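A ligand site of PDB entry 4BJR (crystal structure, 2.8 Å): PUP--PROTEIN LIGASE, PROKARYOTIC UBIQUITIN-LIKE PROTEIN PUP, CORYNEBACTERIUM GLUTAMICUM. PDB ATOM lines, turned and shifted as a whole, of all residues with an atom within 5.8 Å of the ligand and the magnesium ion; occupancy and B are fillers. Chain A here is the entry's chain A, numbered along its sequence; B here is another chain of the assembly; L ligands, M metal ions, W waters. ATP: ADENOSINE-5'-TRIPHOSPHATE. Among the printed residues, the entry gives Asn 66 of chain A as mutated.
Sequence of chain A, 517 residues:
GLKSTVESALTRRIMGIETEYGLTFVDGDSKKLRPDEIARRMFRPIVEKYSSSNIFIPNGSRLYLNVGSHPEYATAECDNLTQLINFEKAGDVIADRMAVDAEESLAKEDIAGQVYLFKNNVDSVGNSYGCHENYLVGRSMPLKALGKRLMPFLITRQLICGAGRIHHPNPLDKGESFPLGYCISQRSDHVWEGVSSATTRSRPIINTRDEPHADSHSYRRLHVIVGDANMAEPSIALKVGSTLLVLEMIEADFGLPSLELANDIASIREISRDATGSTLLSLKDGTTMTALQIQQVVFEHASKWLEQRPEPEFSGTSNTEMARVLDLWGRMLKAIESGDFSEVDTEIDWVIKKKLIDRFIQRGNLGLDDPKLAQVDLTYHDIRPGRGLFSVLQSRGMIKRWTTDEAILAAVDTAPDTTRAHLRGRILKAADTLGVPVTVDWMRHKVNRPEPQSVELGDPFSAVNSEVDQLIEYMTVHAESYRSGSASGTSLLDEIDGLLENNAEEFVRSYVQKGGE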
ATOM      1  N   ILE A  14      -2.756 -16.575 -37.636  1.00  0.00           N
ATOM      2  CA  ILE A  14      -2.554 -16.608 -36.196  1.00  0.00           C
ATOM      3  C   ILE A  14      -3.568 -15.716 -35.491  1.00  0.00           C
ATOM      4  O   ILE A  14      -3.731 -14.551 -35.835  1.00  0.00           O
ATOM      5  CB  ILE A  14      -1.155 -16.153 -35.819  1.00  0.00           C
ATOM      6  CG1 ILE A  14      -0.126 -17.100 -36.403  1.00  0.00           C
ATOM      7  CG2 ILE A  14      -1.013 -16.085 -34.322  1.00  0.00           C
ATOM      8  CD1 ILE A  14      -0.125 -18.424 -35.763  1.00  0.00           C
ATOM      9  N   MET A  15      -4.251 -16.280 -34.513  1.00  0.00           N
ATOM     10  CA  MET A  15      -5.195 -15.516 -33.718  1.00  0.00           C
ATOM     11  C   MET A  15      -5.070 -15.820 -32.242  1.00  0.00           C
ATOM     12  O   MET A  15      -4.756 -16.939 -31.856  1.00  0.00           O
ATOM     13  CB  MET A  15      -6.620 -15.776 -34.186  1.00  0.00           C
ATOM     14  CG  MET A  15      -6.939 -17.215 -34.447  1.00  0.00           C
ATOM     15  SD  MET A  15      -8.616 -17.394 -35.002  1.00  0.00           S
ATOM     16  CE  MET A  15      -8.480 -18.911 -35.905  1.00  0.00           C
ATOM     17  N   GLY A  16      -5.272 -14.813 -31.399  1.00  0.00           N
ATOM     18  CA  GLY A  16      -5.263 -15.018 -29.976  1.00  0.00           C
ATOM     19  C   GLY A  16      -6.325 -14.227 -29.252  1.00  0.00           C
ATOM     20  O   GLY A  16      -6.839 -13.255 -29.780  1.00  0.00           O
ATOM     21  N   ILE A  17      -6.649 -14.649 -28.035  1.00  0.00           N
ATOM     22  CA  ILE A  17      -7.623 -13.936 -27.217  1.00  0.00           C
ATOM     23  C   ILE A  17      -7.055 -13.542 -25.872  1.00  0.00           C
ATOM     24  O   ILE A  17      -6.417 -14.327 -25.200  1.00  0.00           O
ATOM     25  CB  ILE A  17      -8.871 -14.785 -26.992  1.00  0.00           C
ATOM     26  CG1 ILE A  17      -9.573 -15.042 -28.319  1.00  0.00           C
ATOM     27  CG2 ILE A  17      -9.827 -14.104 -26.057  1.00  0.00           C
ATOM     28  CD1 ILE A  17     -10.349 -13.898 -28.829  1.00  0.00           C
ATOM     29  N   GLU A  18      -7.307 -12.299 -25.484  1.00  0.00           N
ATOM     30  CA  GLU A  18      -6.930 -11.816 -24.178  1.00  0.00           C
ATOM     31  C   GLU A  18      -8.158 -11.677 -23.310  1.00  0.00           C
ATOM     32  O   GLU A  18      -9.028 -10.872 -23.605  1.00  0.00           O
ATOM     33  CB  GLU A  18      -6.215 -10.469 -24.285  1.00  0.00           C
ATOM     34  CG  GLU A  18      -4.795 -10.521 -24.780  1.00  0.00           C
ATOM     35  CD  GLU A  18      -4.229  -9.138 -24.989  1.00  0.00           C
ATOM     36  OE1 GLU A  18      -4.293  -8.327 -24.056  1.00  0.00           O
ATOM     37  OE2 GLU A  18      -3.705  -8.868 -26.076  1.00  0.00           O
ATOM     38  N   PHE A  56       4.318 -17.634 -18.164  1.00  0.00           N
ATOM     39  CA  PHE A  56       3.847 -18.422 -19.293  1.00  0.00           C
ATOM     40  C   PHE A  56       3.714 -19.867 -18.855  1.00  0.00           C
ATOM     41  O   PHE A  56       4.650 -20.458 -18.354  1.00  0.00           O
ATOM     42  CB  PHE A  56       4.815 -18.314 -20.456  1.00  0.00           C
ATOM     43  CG  PHE A  56       4.555 -17.162 -21.375  1.00  0.00           C
ATOM     44  CD1 PHE A  56       5.046 -15.908 -21.090  1.00  0.00           C
ATOM     45  CD2 PHE A  56       3.847 -17.338 -22.530  1.00  0.00           C
ATOM     46  CE1 PHE A  56       4.821 -14.861 -21.924  1.00  0.00           C
ATOM     47  CE2 PHE A  56       3.624 -16.293 -23.374  1.00  0.00           C
ATOM     48  CZ  PHE A  56       4.116 -15.051 -23.076  1.00  0.00           C
ATOM     49  N   ARG A  62      -0.262 -17.091 -21.817  1.00  0.00           N
ATOM     50  CA  ARG A  62       0.272 -16.193 -20.820  1.00  0.00           C
ATOM     51  C   ARG A  62      -0.748 -15.956 -19.723  1.00  0.00           C
ATOM     52  O   ARG A  62      -1.887 -15.645 -19.989  1.00  0.00           O
ATOM     53  CB  ARG A  62       0.694 -14.884 -21.466  1.00  0.00           C
ATOM     54  CG  ARG A  62       1.350 -13.900 -20.539  1.00  0.00           C
ATOM     55  CD  ARG A  62       1.739 -12.644 -21.279  1.00  0.00           C
ATOM     56  NE  ARG A  62       2.285 -11.637 -20.386  1.00  0.00           N
ATOM     57  CZ  ARG A  62       2.029 -10.345 -20.487  1.00  0.00           C
ATOM     58  NH1 ARG A  62       1.226  -9.890 -21.431  1.00  0.00           N
ATOM     59  NH2 ARG A  62       2.567  -9.489 -19.628  1.00  0.00           N
ATOM     60  N   TYR A  64      -1.347 -13.820 -16.157  1.00  0.00           N
ATOM     61  CA  TYR A  64      -0.781 -12.780 -15.320  1.00  0.00           C
ATOM     62  C   TYR A  64      -1.780 -11.933 -14.569  1.00  0.00           C
ATOM     63  O   TYR A  64      -2.954 -11.969 -14.834  1.00  0.00           O
ATOM     64  CB  TYR A  64       0.120 -11.851 -16.134  1.00  0.00           C
ATOM     65  CG  TYR A  64      -0.514 -11.082 -17.267  1.00  0.00           C
ATOM     66  CD1 TYR A  64      -0.929 -11.715 -18.413  1.00  0.00           C
ATOM     67  CD2 TYR A  64      -0.636  -9.706 -17.199  1.00  0.00           C
ATOM     68  CE1 TYR A  64      -1.468 -10.994 -19.457  1.00  0.00           C
ATOM     69  CE2 TYR A  64      -1.175  -8.996 -18.230  1.00  0.00           C
ATOM     70  CZ  TYR A  64      -1.592  -9.640 -19.353  1.00  0.00           C
ATOM     71  OH  TYR A  64      -2.128  -8.932 -20.393  1.00  0.00           O
ATOM     72  N   ASN A  66      -3.188  -8.406 -13.756  1.00  0.00           N
ATOM     73  CA  ASN A  66      -3.329  -7.122 -14.426  1.00  0.00           C
ATOM     74  C   ASN A  66      -3.062  -5.932 -13.544  1.00  0.00           C
ATOM     75  O   ASN A  66      -3.096  -6.007 -12.330  1.00  0.00           O
ATOM     76  CB  ASN A  66      -4.738  -6.988 -14.983  1.00  0.00           C
ATOM     77  CG  ASN A  66      -4.759  -6.547 -16.406  1.00  0.00           C
ATOM     78  OD1 ASN A  66      -3.717  -6.388 -17.029  1.00  0.00           O
ATOM     79  ND2 ASN A  66      -5.948  -6.341 -16.928  1.00  0.00           N
ATOM     80  N   GLU A  72      -5.641 -12.178 -15.801  1.00  0.00           N
ATOM     81  CA  GLU A  72      -5.717 -12.133 -17.251  1.00  0.00           C
ATOM     82  C   GLU A  72      -5.073 -13.354 -17.883  1.00  0.00           C
ATOM     83  O   GLU A  72      -3.973 -13.758 -17.546  1.00  0.00           O
ATOM     84  CB  GLU A  72      -5.058 -10.869 -17.779  1.00  0.00           C
ATOM     85  CG  GLU A  72      -5.080 -10.777 -19.288  1.00  0.00           C
ATOM     86  CD  GLU A  72      -4.881  -9.377 -19.803  1.00  0.00           C
ATOM     87  OE1 GLU A  72      -5.105  -8.417 -19.041  1.00  0.00           O
ATOM     88  OE2 GLU A  72      -4.479  -9.232 -20.972  1.00  0.00           O
ATOM     89  N   ALA A  74      -4.110 -14.885 -21.625  1.00  0.00           N
ATOM     90  CA  ALA A  74      -3.938 -14.630 -23.039  1.00  0.00           C
ATOM     91  C   ALA A  74      -3.622 -15.936 -23.714  1.00  0.00           C
ATOM     92  O   ALA A  74      -2.663 -16.605 -23.359  1.00  0.00           O
ATOM     93  CB  ALA A  74      -2.851 -13.628 -23.277  1.00  0.00           C
ATOM     94  N   THR A  75      -4.427 -16.307 -24.695  1.00  0.00           N
ATOM     95  CA  THR A  75      -4.283 -17.605 -25.303  1.00  0.00           C
ATOM     96  C   THR A  75      -3.004 -17.727 -26.055  1.00  0.00           C
ATOM     97  O   THR A  75      -2.460 -16.758 -26.554  1.00  0.00           O
ATOM     98  CB  THR A  75      -5.419 -17.914 -26.273  1.00  0.00           C
ATOM     99  OG1 THR A  75      -5.334 -17.019 -27.392  1.00  0.00           O
ATOM    100  CG2 THR A  75      -6.735 -17.747 -25.604  1.00  0.00           C
ATOM    101  N   ALA A  76      -2.527 -18.954 -26.140  1.00  0.00           N
ATOM    102  CA  ALA A  76      -1.433 -19.280 -27.007  1.00  0.00           C
ATOM    103  C   ALA A  76      -1.880 -19.050 -28.429  1.00  0.00           C
ATOM    104  O   ALA A  76      -3.067 -19.053 -28.705  1.00  0.00           O
ATOM    105  CB  ALA A  76      -1.013 -20.701 -26.802  1.00  0.00           C
ATOM    106  N   GLU A  77      -0.930 -18.814 -29.317  1.00  0.00           N
ATOM    107  CA  GLU A  77      -1.259 -18.576 -30.708  1.00  0.00           C
ATOM    108  C   GLU A  77      -1.972 -19.776 -31.288  1.00  0.00           C
ATOM    109  O   GLU A  77      -1.547 -20.914 -31.110  1.00  0.00           O
ATOM    110  CB  GLU A  77      -0.004 -18.288 -31.522  1.00  0.00           C
ATOM    111  CG  GLU A  77       0.848 -17.193 -30.955  1.00  0.00           C
ATOM    112  CD  GLU A  77       1.941 -17.720 -30.064  1.00  0.00           C
ATOM    113  OE1 GLU A  77       1.664 -18.593 -29.236  1.00  0.00           O
ATOM    114  OE2 GLU A  77       3.081 -17.241 -30.177  1.00  0.00           O
ATOM    115  N   CYS A  78      -3.078 -19.521 -31.967  1.00  0.00           N
ATOM    116  CA  CYS A  78      -3.871 -20.562 -32.592  1.00  0.00           C
ATOM    117  C   CYS A  78      -4.102 -20.223 -34.062  1.00  0.00           C
ATOM    118  O   CYS A  78      -4.322 -19.070 -34.409  1.00  0.00           O
ATOM    119  CB  CYS A  78      -5.204 -20.729 -31.857  1.00  0.00           C
ATOM    120  SG  CYS A  78      -5.086 -21.274 -30.163  1.00  0.00           S
ATOM    121  N   ASN A 134      -6.941 -10.723 -31.148  1.00  0.00           N
ATOM    122  CA  ASN A 134      -5.735 -10.474 -31.935  1.00  0.00           C
ATOM    123  C   ASN A 134      -5.674 -11.292 -33.207  1.00  0.00           C
ATOM    124  O   ASN A 134      -5.742 -12.516 -33.159  1.00  0.00           O
ATOM    125  CB  ASN A 134      -4.501 -10.748 -31.080  1.00  0.00           C
ATOM    126  CG  ASN A 134      -4.508  -9.964 -29.807  1.00  0.00           C
ATOM    127  OD1 ASN A 134      -3.948  -8.882 -29.742  1.00  0.00           O
ATOM    128  ND2 ASN A 134      -5.140 -10.502 -28.788  1.00  0.00           N
ATOM    129  N   TYR A 135      -5.503 -10.622 -34.339  1.00  0.00           N
ATOM    130  CA  TYR A 135      -5.405 -11.298 -35.631  1.00  0.00           C
ATOM    131  C   TYR A 135      -4.141 -10.943 -36.393  1.00  0.00           C
ATOM    132  O   TYR A 135      -3.828  -9.777 -36.573  1.00  0.00           O
ATOM    133  CB  TYR A 135      -6.611 -10.947 -36.495  1.00  0.00           C
ATOM    134  CG  TYR A 135      -7.956 -11.169 -35.848  1.00  0.00           C
ATOM    135  CD1 TYR A 135      -8.602 -12.387 -35.950  1.00  0.00           C
ATOM    136  CD2 TYR A 135      -8.578 -10.153 -35.165  1.00  0.00           C
ATOM    137  CE1 TYR A 135      -9.829 -12.580 -35.360  1.00  0.00           C
ATOM    138  CE2 TYR A 135      -9.799 -10.337 -34.576  1.00  0.00           C
ATOM    139  CZ  TYR A 135     -10.418 -11.549 -34.672  1.00  0.00           C
ATOM    140  OH  TYR A 135     -11.642 -11.732 -34.073  1.00  0.00           O
ATOM    141  N   LEU A 136      -3.409 -11.942 -36.858  1.00  0.00           N
ATOM    142  CA  LEU A 136      -2.251 -11.698 -37.689  1.00  0.00           C
ATOM    143  C   LEU A 136      -2.655 -11.182 -39.043  1.00  0.00           C
ATOM    144  O   LEU A 136      -3.596 -11.693 -39.642  1.00  0.00           O
ATOM    145  CB  LEU A 136      -1.406 -12.966 -37.843  1.00  0.00           C
ATOM    146  CG  LEU A 136      -0.247 -12.919 -38.834  1.00  0.00           C
ATOM    147  CD1 LEU A 136       0.961 -13.591 -38.261  1.00  0.00           C
ATOM    148  CD2 LEU A 136      -0.635 -13.586 -40.125  1.00  0.00           C
ATOM    149  N   ASP A 210       0.756  -1.784 -32.593  1.00  0.00           N
ATOM    150  CA  ASP A 210       1.456  -2.467 -31.513  1.00  0.00           C
ATOM    151  C   ASP A 210       2.292  -3.619 -32.012  1.00  0.00           C
ATOM    152  O   ASP A 210       2.076  -4.094 -33.116  1.00  0.00           O
ATOM    153  CB  ASP A 210       0.478  -2.966 -30.451  1.00  0.00           C
ATOM    154  CG  ASP A 210       1.119  -3.099 -29.101  1.00  0.00           C
ATOM    155  OD1 ASP A 210       2.347  -3.056 -29.044  1.00  0.00           O
ATOM    156  OD2 ASP A 210       0.406  -3.272 -28.108  1.00  0.00           O
ATOM    157  N   GLU A 211       3.253  -4.038 -31.212  1.00  0.00           N
ATOM    158  CA  GLU A 211       4.204  -5.048 -31.645  1.00  0.00           C
ATOM    159  C   GLU A 211       3.548  -6.330 -32.097  1.00  0.00           C
ATOM    160  O   GLU A 211       2.726  -6.894 -31.390  1.00  0.00           O
ATOM    161  CB  GLU A 211       5.189  -5.366 -30.531  1.00  0.00           C
ATOM    162  CG  GLU A 211       4.667  -5.223 -29.139  1.00  0.00           C
ATOM    163  CD  GLU A 211       5.750  -5.416 -28.099  1.00  0.00           C
ATOM    164  OE1 GLU A 211       6.753  -6.086 -28.399  1.00  0.00           O
ATOM    165  OE2 GLU A 211       5.596  -4.900 -26.980  1.00  0.00           O
ATOM    166  N   PRO A 212       3.941  -6.814 -33.283  1.00  0.00           N
ATOM    167  CA  PRO A 212       3.376  -7.959 -33.982  1.00  0.00           C
ATOM    168  C   PRO A 212       3.594  -9.268 -33.264  1.00  0.00           C
ATOM    169  O   PRO A 212       2.777 -10.160 -33.419  1.00  0.00           O
ATOM    170  CB  PRO A 212       4.115  -7.944 -35.316  1.00  0.00           C
ATOM    171  CG  PRO A 212       5.324  -7.200 -35.063  1.00  0.00           C
ATOM    172  CD  PRO A 212       4.952  -6.150 -34.107  1.00  0.00           C
ATOM    173  N   HIS A 213       4.707  -9.382 -32.539  1.00  0.00           N
ATOM    174  CA  HIS A 213       5.115 -10.640 -31.927  1.00  0.00           C
ATOM    175  C   HIS A 213       5.405 -11.641 -33.033  1.00  0.00           C
ATOM    176  O   HIS A 213       5.308 -12.854 -32.868  1.00  0.00           O
ATOM    177  CB  HIS A 213       4.056 -11.161 -30.946  1.00  0.00           C
ATOM    178  CG  HIS A 213       3.887 -10.296 -29.735  1.00  0.00           C
ATOM    179  ND1 HIS A 213       2.662 -10.107 -29.131  1.00  0.00           N
ATOM    180  CD2 HIS A 213       4.783  -9.608 -28.996  1.00  0.00           C
ATOM    181  CE1 HIS A 213       2.809  -9.312 -28.093  1.00  0.00           C
ATOM    182  NE2 HIS A 213       4.093  -8.993 -27.983  1.00  0.00           N
ATOM    183  N   ALA A 214       5.732 -11.074 -34.185  1.00  0.00           N
ATOM    184  CA  ALA A 214       6.147 -11.788 -35.359  1.00  0.00           C
ATOM    185  C   ALA A 214       7.159 -10.931 -36.096  1.00  0.00           C
ATOM    186  O   ALA A 214       7.344  -9.773 -35.738  1.00  0.00           O
ATOM    187  CB  ALA A 214       4.988 -12.115 -36.237  1.00  0.00           C
ATOM    188  N   ARG A 220       1.936  -7.792 -39.226  1.00  0.00           N
ATOM    189  CA  ARG A 220       1.403  -6.932 -38.179  1.00  0.00           C
ATOM    190  C   ARG A 220       0.390  -7.691 -37.346  1.00  0.00           C
ATOM    191  O   ARG A 220      -0.126  -8.716 -37.761  1.00  0.00           O
ATOM    192  CB  ARG A 220       0.730  -5.690 -38.755  1.00  0.00           C
ATOM    193  CG  ARG A 220       1.668  -4.671 -39.303  1.00  0.00           C
ATOM    194  CD  ARG A 220       0.894  -3.453 -39.701  1.00  0.00           C
ATOM    195  NE  ARG A 220       1.691  -2.514 -40.462  1.00  0.00           N
ATOM    196  CZ  ARG A 220       2.320  -1.476 -39.934  1.00  0.00           C
ATOM    197  NH1 ARG A 220       2.246  -1.247 -38.637  1.00  0.00           N
ATOM    198  NH2 ARG A 220       3.024  -0.668 -40.704  1.00  0.00           N
ATOM    199  N   ARG A 221       0.113  -7.163 -36.158  1.00  0.00           N
ATOM    200  CA  ARG A 221      -0.917  -7.718 -35.299  1.00  0.00           C
ATOM    201  C   ARG A 221      -2.069  -6.751 -35.178  1.00  0.00           C
ATOM    202  O   ARG A 221      -1.884  -5.583 -34.865  1.00  0.00           O
ATOM    203  CB  ARG A 221      -0.343  -8.033 -33.919  1.00  0.00           C
ATOM    204  CG  ARG A 221      -1.208  -8.901 -33.065  1.00  0.00           C
ATOM    205  CD  ARG A 221      -0.539  -9.269 -31.754  1.00  0.00           C
ATOM    206  NE  ARG A 221       0.352  -8.225 -31.271  1.00  0.00           N
ATOM    207  CZ  ARG A 221       0.150  -7.522 -30.173  1.00  0.00           C
ATOM    208  NH1 ARG A 221      -0.925  -7.740 -29.440  1.00  0.00           N
ATOM    209  NH2 ARG A 221       1.018  -6.610 -29.807  1.00  0.00           N
ATOM    210  N   HIS A 223      -5.383  -5.546 -33.334  1.00  0.00           N
ATOM    211  CA  HIS A 223      -5.919  -5.610 -31.987  1.00  0.00           C
ATOM    212  C   HIS A 223      -7.314  -5.024 -31.936  1.00  0.00           C
ATOM    213  O   HIS A 223      -7.534  -3.883 -32.302  1.00  0.00           O
ATOM    214  CB  HIS A 223      -5.008  -4.853 -31.025  1.00  0.00           C
ATOM    215  CG  HIS A 223      -5.292  -5.105 -29.578  1.00  0.00           C
ATOM    216  ND1 HIS A 223      -5.068  -6.326 -28.983  1.00  0.00           N
ATOM    217  CD2 HIS A 223      -5.786  -4.297 -28.615  1.00  0.00           C
ATOM    218  CE1 HIS A 223      -5.409  -6.257 -27.715  1.00  0.00           C
ATOM    219  NE2 HIS A 223      -5.849  -5.038 -27.459  1.00  0.00           N
ATOM    220  N   ARG A 420       3.432 -21.802 -33.342  1.00  0.00           N
ATOM    221  CA  ARG A 420       4.685 -21.625 -32.618  1.00  0.00           C
ATOM    222  C   ARG A 420       4.592 -21.978 -31.150  1.00  0.00           C
ATOM    223  O   ARG A 420       5.583 -22.374 -30.538  1.00  0.00           O
ATOM    224  CB  ARG A 420       5.147 -20.173 -32.775  1.00  0.00           C
ATOM    225  CG  ARG A 420       6.059 -19.665 -31.687  1.00  0.00           C
ATOM    226  CD  ARG A 420       6.528 -18.282 -31.997  1.00  0.00           C
ATOM    227  NE  ARG A 420       5.486 -17.280 -31.873  1.00  0.00           N
ATOM    228  CZ  ARG A 420       5.640 -16.015 -32.246  1.00  0.00           C
ATOM    229  NH1 ARG A 420       6.791 -15.613 -32.752  1.00  0.00           N
ATOM    230  NH2 ARG A 420       4.656 -15.147 -32.109  1.00  0.00           N
ATOM    231  N   TRP A 442       6.659 -14.177 -26.113  1.00  0.00           N
ATOM    232  CA  TRP A 442       5.991 -14.634 -27.314  1.00  0.00           C
ATOM    233  C   TRP A 442       7.028 -14.976 -28.373  1.00  0.00           C
ATOM    234  O   TRP A 442       7.013 -16.048 -28.945  1.00  0.00           O
ATOM    235  CB  TRP A 442       5.021 -13.590 -27.846  1.00  0.00           C
ATOM    236  CG  TRP A 442       3.872 -13.322 -26.940  1.00  0.00           C
ATOM    237  CD1 TRP A 442       3.643 -12.182 -26.249  1.00  0.00           C
ATOM    238  CD2 TRP A 442       2.814 -14.209 -26.623  1.00  0.00           C
ATOM    239  NE1 TRP A 442       2.493 -12.301 -25.516  1.00  0.00           N
ATOM    240  CE2 TRP A 442       1.967 -13.542 -25.728  1.00  0.00           C
ATOM    241  CE3 TRP A 442       2.489 -15.504 -27.012  1.00  0.00           C
ATOM    242  CZ2 TRP A 442       0.823 -14.128 -25.223  1.00  0.00           C
ATOM    243  CZ3 TRP A 442       1.351 -16.081 -26.507  1.00  0.00           C
ATOM    244  CH2 TRP A 442       0.531 -15.396 -25.619  1.00  0.00           C
ATOM    245  N   PRO A 460       5.519 -17.314 -36.146  1.00  0.00           N
ATOM    246  CA  PRO A 460       4.404 -17.827 -35.352  1.00  0.00           C
ATOM    247  C   PRO A 460       3.858 -19.124 -35.907  1.00  0.00           C
ATOM    248  O   PRO A 460       3.365 -19.952 -35.160  1.00  0.00           O
ATOM    249  CB  PRO A 460       3.371 -16.706 -35.430  1.00  0.00           C
ATOM    250  CG  PRO A 460       3.721 -15.951 -36.616  1.00  0.00           C
ATOM    251  CD  PRO A 460       5.184 -16.008 -36.737  1.00  0.00           C
ATOM    252  N   GLU B 517      -6.570  -1.871 -18.670  1.00  0.00           N
ATOM    253  CA  GLU B 517      -6.071  -1.507 -20.006  1.00  0.00           C
ATOM    254  C   GLU B 517      -7.071  -0.715 -20.832  1.00  0.00           C
ATOM    255  O   GLU B 517      -6.712   0.239 -21.516  1.00  0.00           O
ATOM    256  CB  GLU B 517      -5.633  -2.763 -20.773  1.00  0.00           C
ATOM    257  CG  GLU B 517      -5.349  -2.488 -22.246  1.00  0.00           C
ATOM    258  CD  GLU B 517      -4.152  -1.584 -22.507  1.00  0.00           C
ATOM    259  OE1 GLU B 517      -3.090  -1.751 -21.859  1.00  0.00           O
ATOM    260  OE2 GLU B 517      -4.290  -0.653 -23.335  1.00  0.00           O
HETATM  261  PG  ATP L   1       1.031  -5.925 -22.619  1.00  0.00           P
HETATM  262  O1G ATP L   1       1.265  -7.047 -21.649  1.00  0.00           O
HETATM  263  O2G ATP L   1      -0.301  -5.247 -22.454  1.00  0.00           O
HETATM  264  O3G ATP L   1       2.189  -4.993 -22.801  1.00  0.00           O
HETATM  265  PB  ATP L   1      -0.365  -7.383 -24.541  1.00  0.00           P
HETATM  266  O1B ATP L   1      -1.369  -7.397 -23.419  1.00  0.00           O
HETATM  267  O2B ATP L   1      -0.727  -6.763 -25.864  1.00  0.00           O
HETATM  268  O3B ATP L   1       0.969  -6.656 -24.038  1.00  0.00           O
HETATM  269  PA  ATP L   1      -0.519 -10.187 -24.320  1.00  0.00           P
HETATM  270  O1A ATP L   1       0.558 -11.206 -24.219  1.00  0.00           O
HETATM  271  O2A ATP L   1      -1.405  -9.929 -23.149  1.00  0.00           O
HETATM  272  O3A ATP L   1       0.200  -8.854 -24.826  1.00  0.00           O
HETATM  273  O5' ATP L   1      -1.436 -10.540 -25.581  1.00  0.00           O
HETATM  274  C5' ATP L   1      -0.861 -11.308 -26.615  1.00  0.00           C
HETATM  275  C4' ATP L   1      -1.911 -11.911 -27.520  1.00  0.00           C
HETATM  276  O4' ATP L   1      -1.436 -11.843 -28.864  1.00  0.00           O
HETATM  277  C3' ATP L   1      -2.090 -13.366 -27.199  1.00  0.00           C
HETATM  278  O3' ATP L   1      -3.488 -13.629 -27.161  1.00  0.00           O
HETATM  279  C2' ATP L   1      -1.491 -14.117 -28.357  1.00  0.00           C
HETATM  280  O2' ATP L   1      -2.301 -15.243 -28.619  1.00  0.00           O
HETATM  281  C1' ATP L   1      -1.551 -13.114 -29.475  1.00  0.00           C
HETATM  282  N9  ATP L   1      -0.438 -13.251 -30.429  1.00  0.00           N
HETATM  283  C8  ATP L   1       0.826 -13.574 -30.148  1.00  0.00           C
HETATM  284  N7  ATP L   1       1.578 -13.597 -31.268  1.00  0.00           N
HETATM  285  C5  ATP L   1       0.786 -13.272 -32.288  1.00  0.00           C
HETATM  286  C6  ATP L   1       0.928 -13.107 -33.744  1.00  0.00           C
HETATM  287  N6  ATP L   1       2.105 -13.301 -34.362  1.00  0.00           N
HETATM  288  N1  ATP L   1      -0.173 -12.761 -34.441  1.00  0.00           N
HETATM  289  C2  ATP L   1      -1.355 -12.576 -33.855  1.00  0.00           C
HETATM  290  N3  ATP L   1      -1.556 -12.706 -32.539  1.00  0.00           N
HETATM  291  C4  ATP L   1      -0.548 -13.048 -31.731  1.00  0.00           C
HETATM  292 MG    MG M   1      -2.643  -8.418 -22.276  1.00  0.00          MG
HETATM  293  O   HOH W   1       3.175  -6.803 -20.186  1.00  0.00           O
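O of Thr 75 is in hydrogen-bond range of O2' of the ligand, at 2.6 Å. NE1 of Trp 442 sits at hydrogen-bond distance from O1A of the ligand (2.6 Å). NH1 of Arg 62 lies within salt-bridge range of O1G of the ligand (2.9 Å). A nitrogen (N6) of the ligand is in hydrogen-bond range of the backbone carbonyl oxygen of Pro 212. An oxygen (O3') of the ligand sits at hydrogen-bond distance from the backbone NH of Ile 17 (3.4 Å). O2B of the ligand is in salt-bridge range of NH1 of Arg 221.
The side-chain carboxylate (OE1) of Glu 72 sits at hydrogen-bond distance from the side-chain amide nitrogen (ND2) of Asn 66, at 3.1 Å. The backbone NH (N) of Asn 134 lies within hydrogen-bond range of the backbone carbonyl oxygen (O) of Gly 16. O of His 213 sits at hydrogen-bond distance from NH2 of Arg 420 (2.5 Å). The backbone NH of Arg 420 is in hydrogen-bond range of the backbone carbonyl oxygen of Pro 460, at 2.6 Å. The guanidinium group of Arg 221 is in hydrogen-bond range of the side-chain amide oxygen of Asn 134 (3.2 Å). OD2 of Asp 210 lies within salt-bridge range of NH2 of Arg 221, at 3.8 Å. The guanidinium group (NE) of Arg 221 lies within hydrogen-bond range of the backbone carbonyl oxygen (O) of Glu 211, at 2.7 Å. The backbone carbonyl oxygen (O) of Ala 76 is in hydrogen-bond range of the side-chain sulfur (SG) of Cys 78, at 3.3 Å.
CG2 of Ile 14 touches N1 of the ligand, 3.4 Å away. Gly 16 touches the ligand. Ala 74 touches the ligand (CB to O3', 3.9 Å). Ala 76 touches the ligand (C to O2', 3.8 Å). CG of Glu 77 touches N7 of the ligand (3.7 Å). Asn 134 touches the ligand. CB of Leu 136 touches N1 of the ligand, 3.6 Å away. His 213 touches the ligand (CB to N7, 3.5 Å). CB of Ala 214 touches N6 of the ligand, 3.6 Å away. NH2 of Arg 420 touches N7 of the ligand, 3.5 Å away. CB of Pro 460 touches N6 of the ligand (3.8 Å). Hydrophobic or aromatic side chains within 4 Å of the ligand: Ile 14, Tyr 64, Ala 74, Leu 136, His 213, Ala 214, Trp 442 and Pro 460. Of the 30 residues printed, 20 come within 4 Å of the ligand. Along chain A the residues within 4 Å of the ligand span positions 14 to 460.
The nearest printed residue that does not touch the magnesium ion is Arg 62 (4.2 Å).
The magnesium ion is bound by O1B of the ligand (2.0 Å), OH of Tyr 64 (2.0 Å), O2A of the ligand (2.1 Å), OE2 of Glu 72 (2.4 Å) and OE1 of Glu 18 (2.4 Å).
Water W1 lies within hydrogen-bond range of O1G of the ligand and NH2 of Arg 62.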
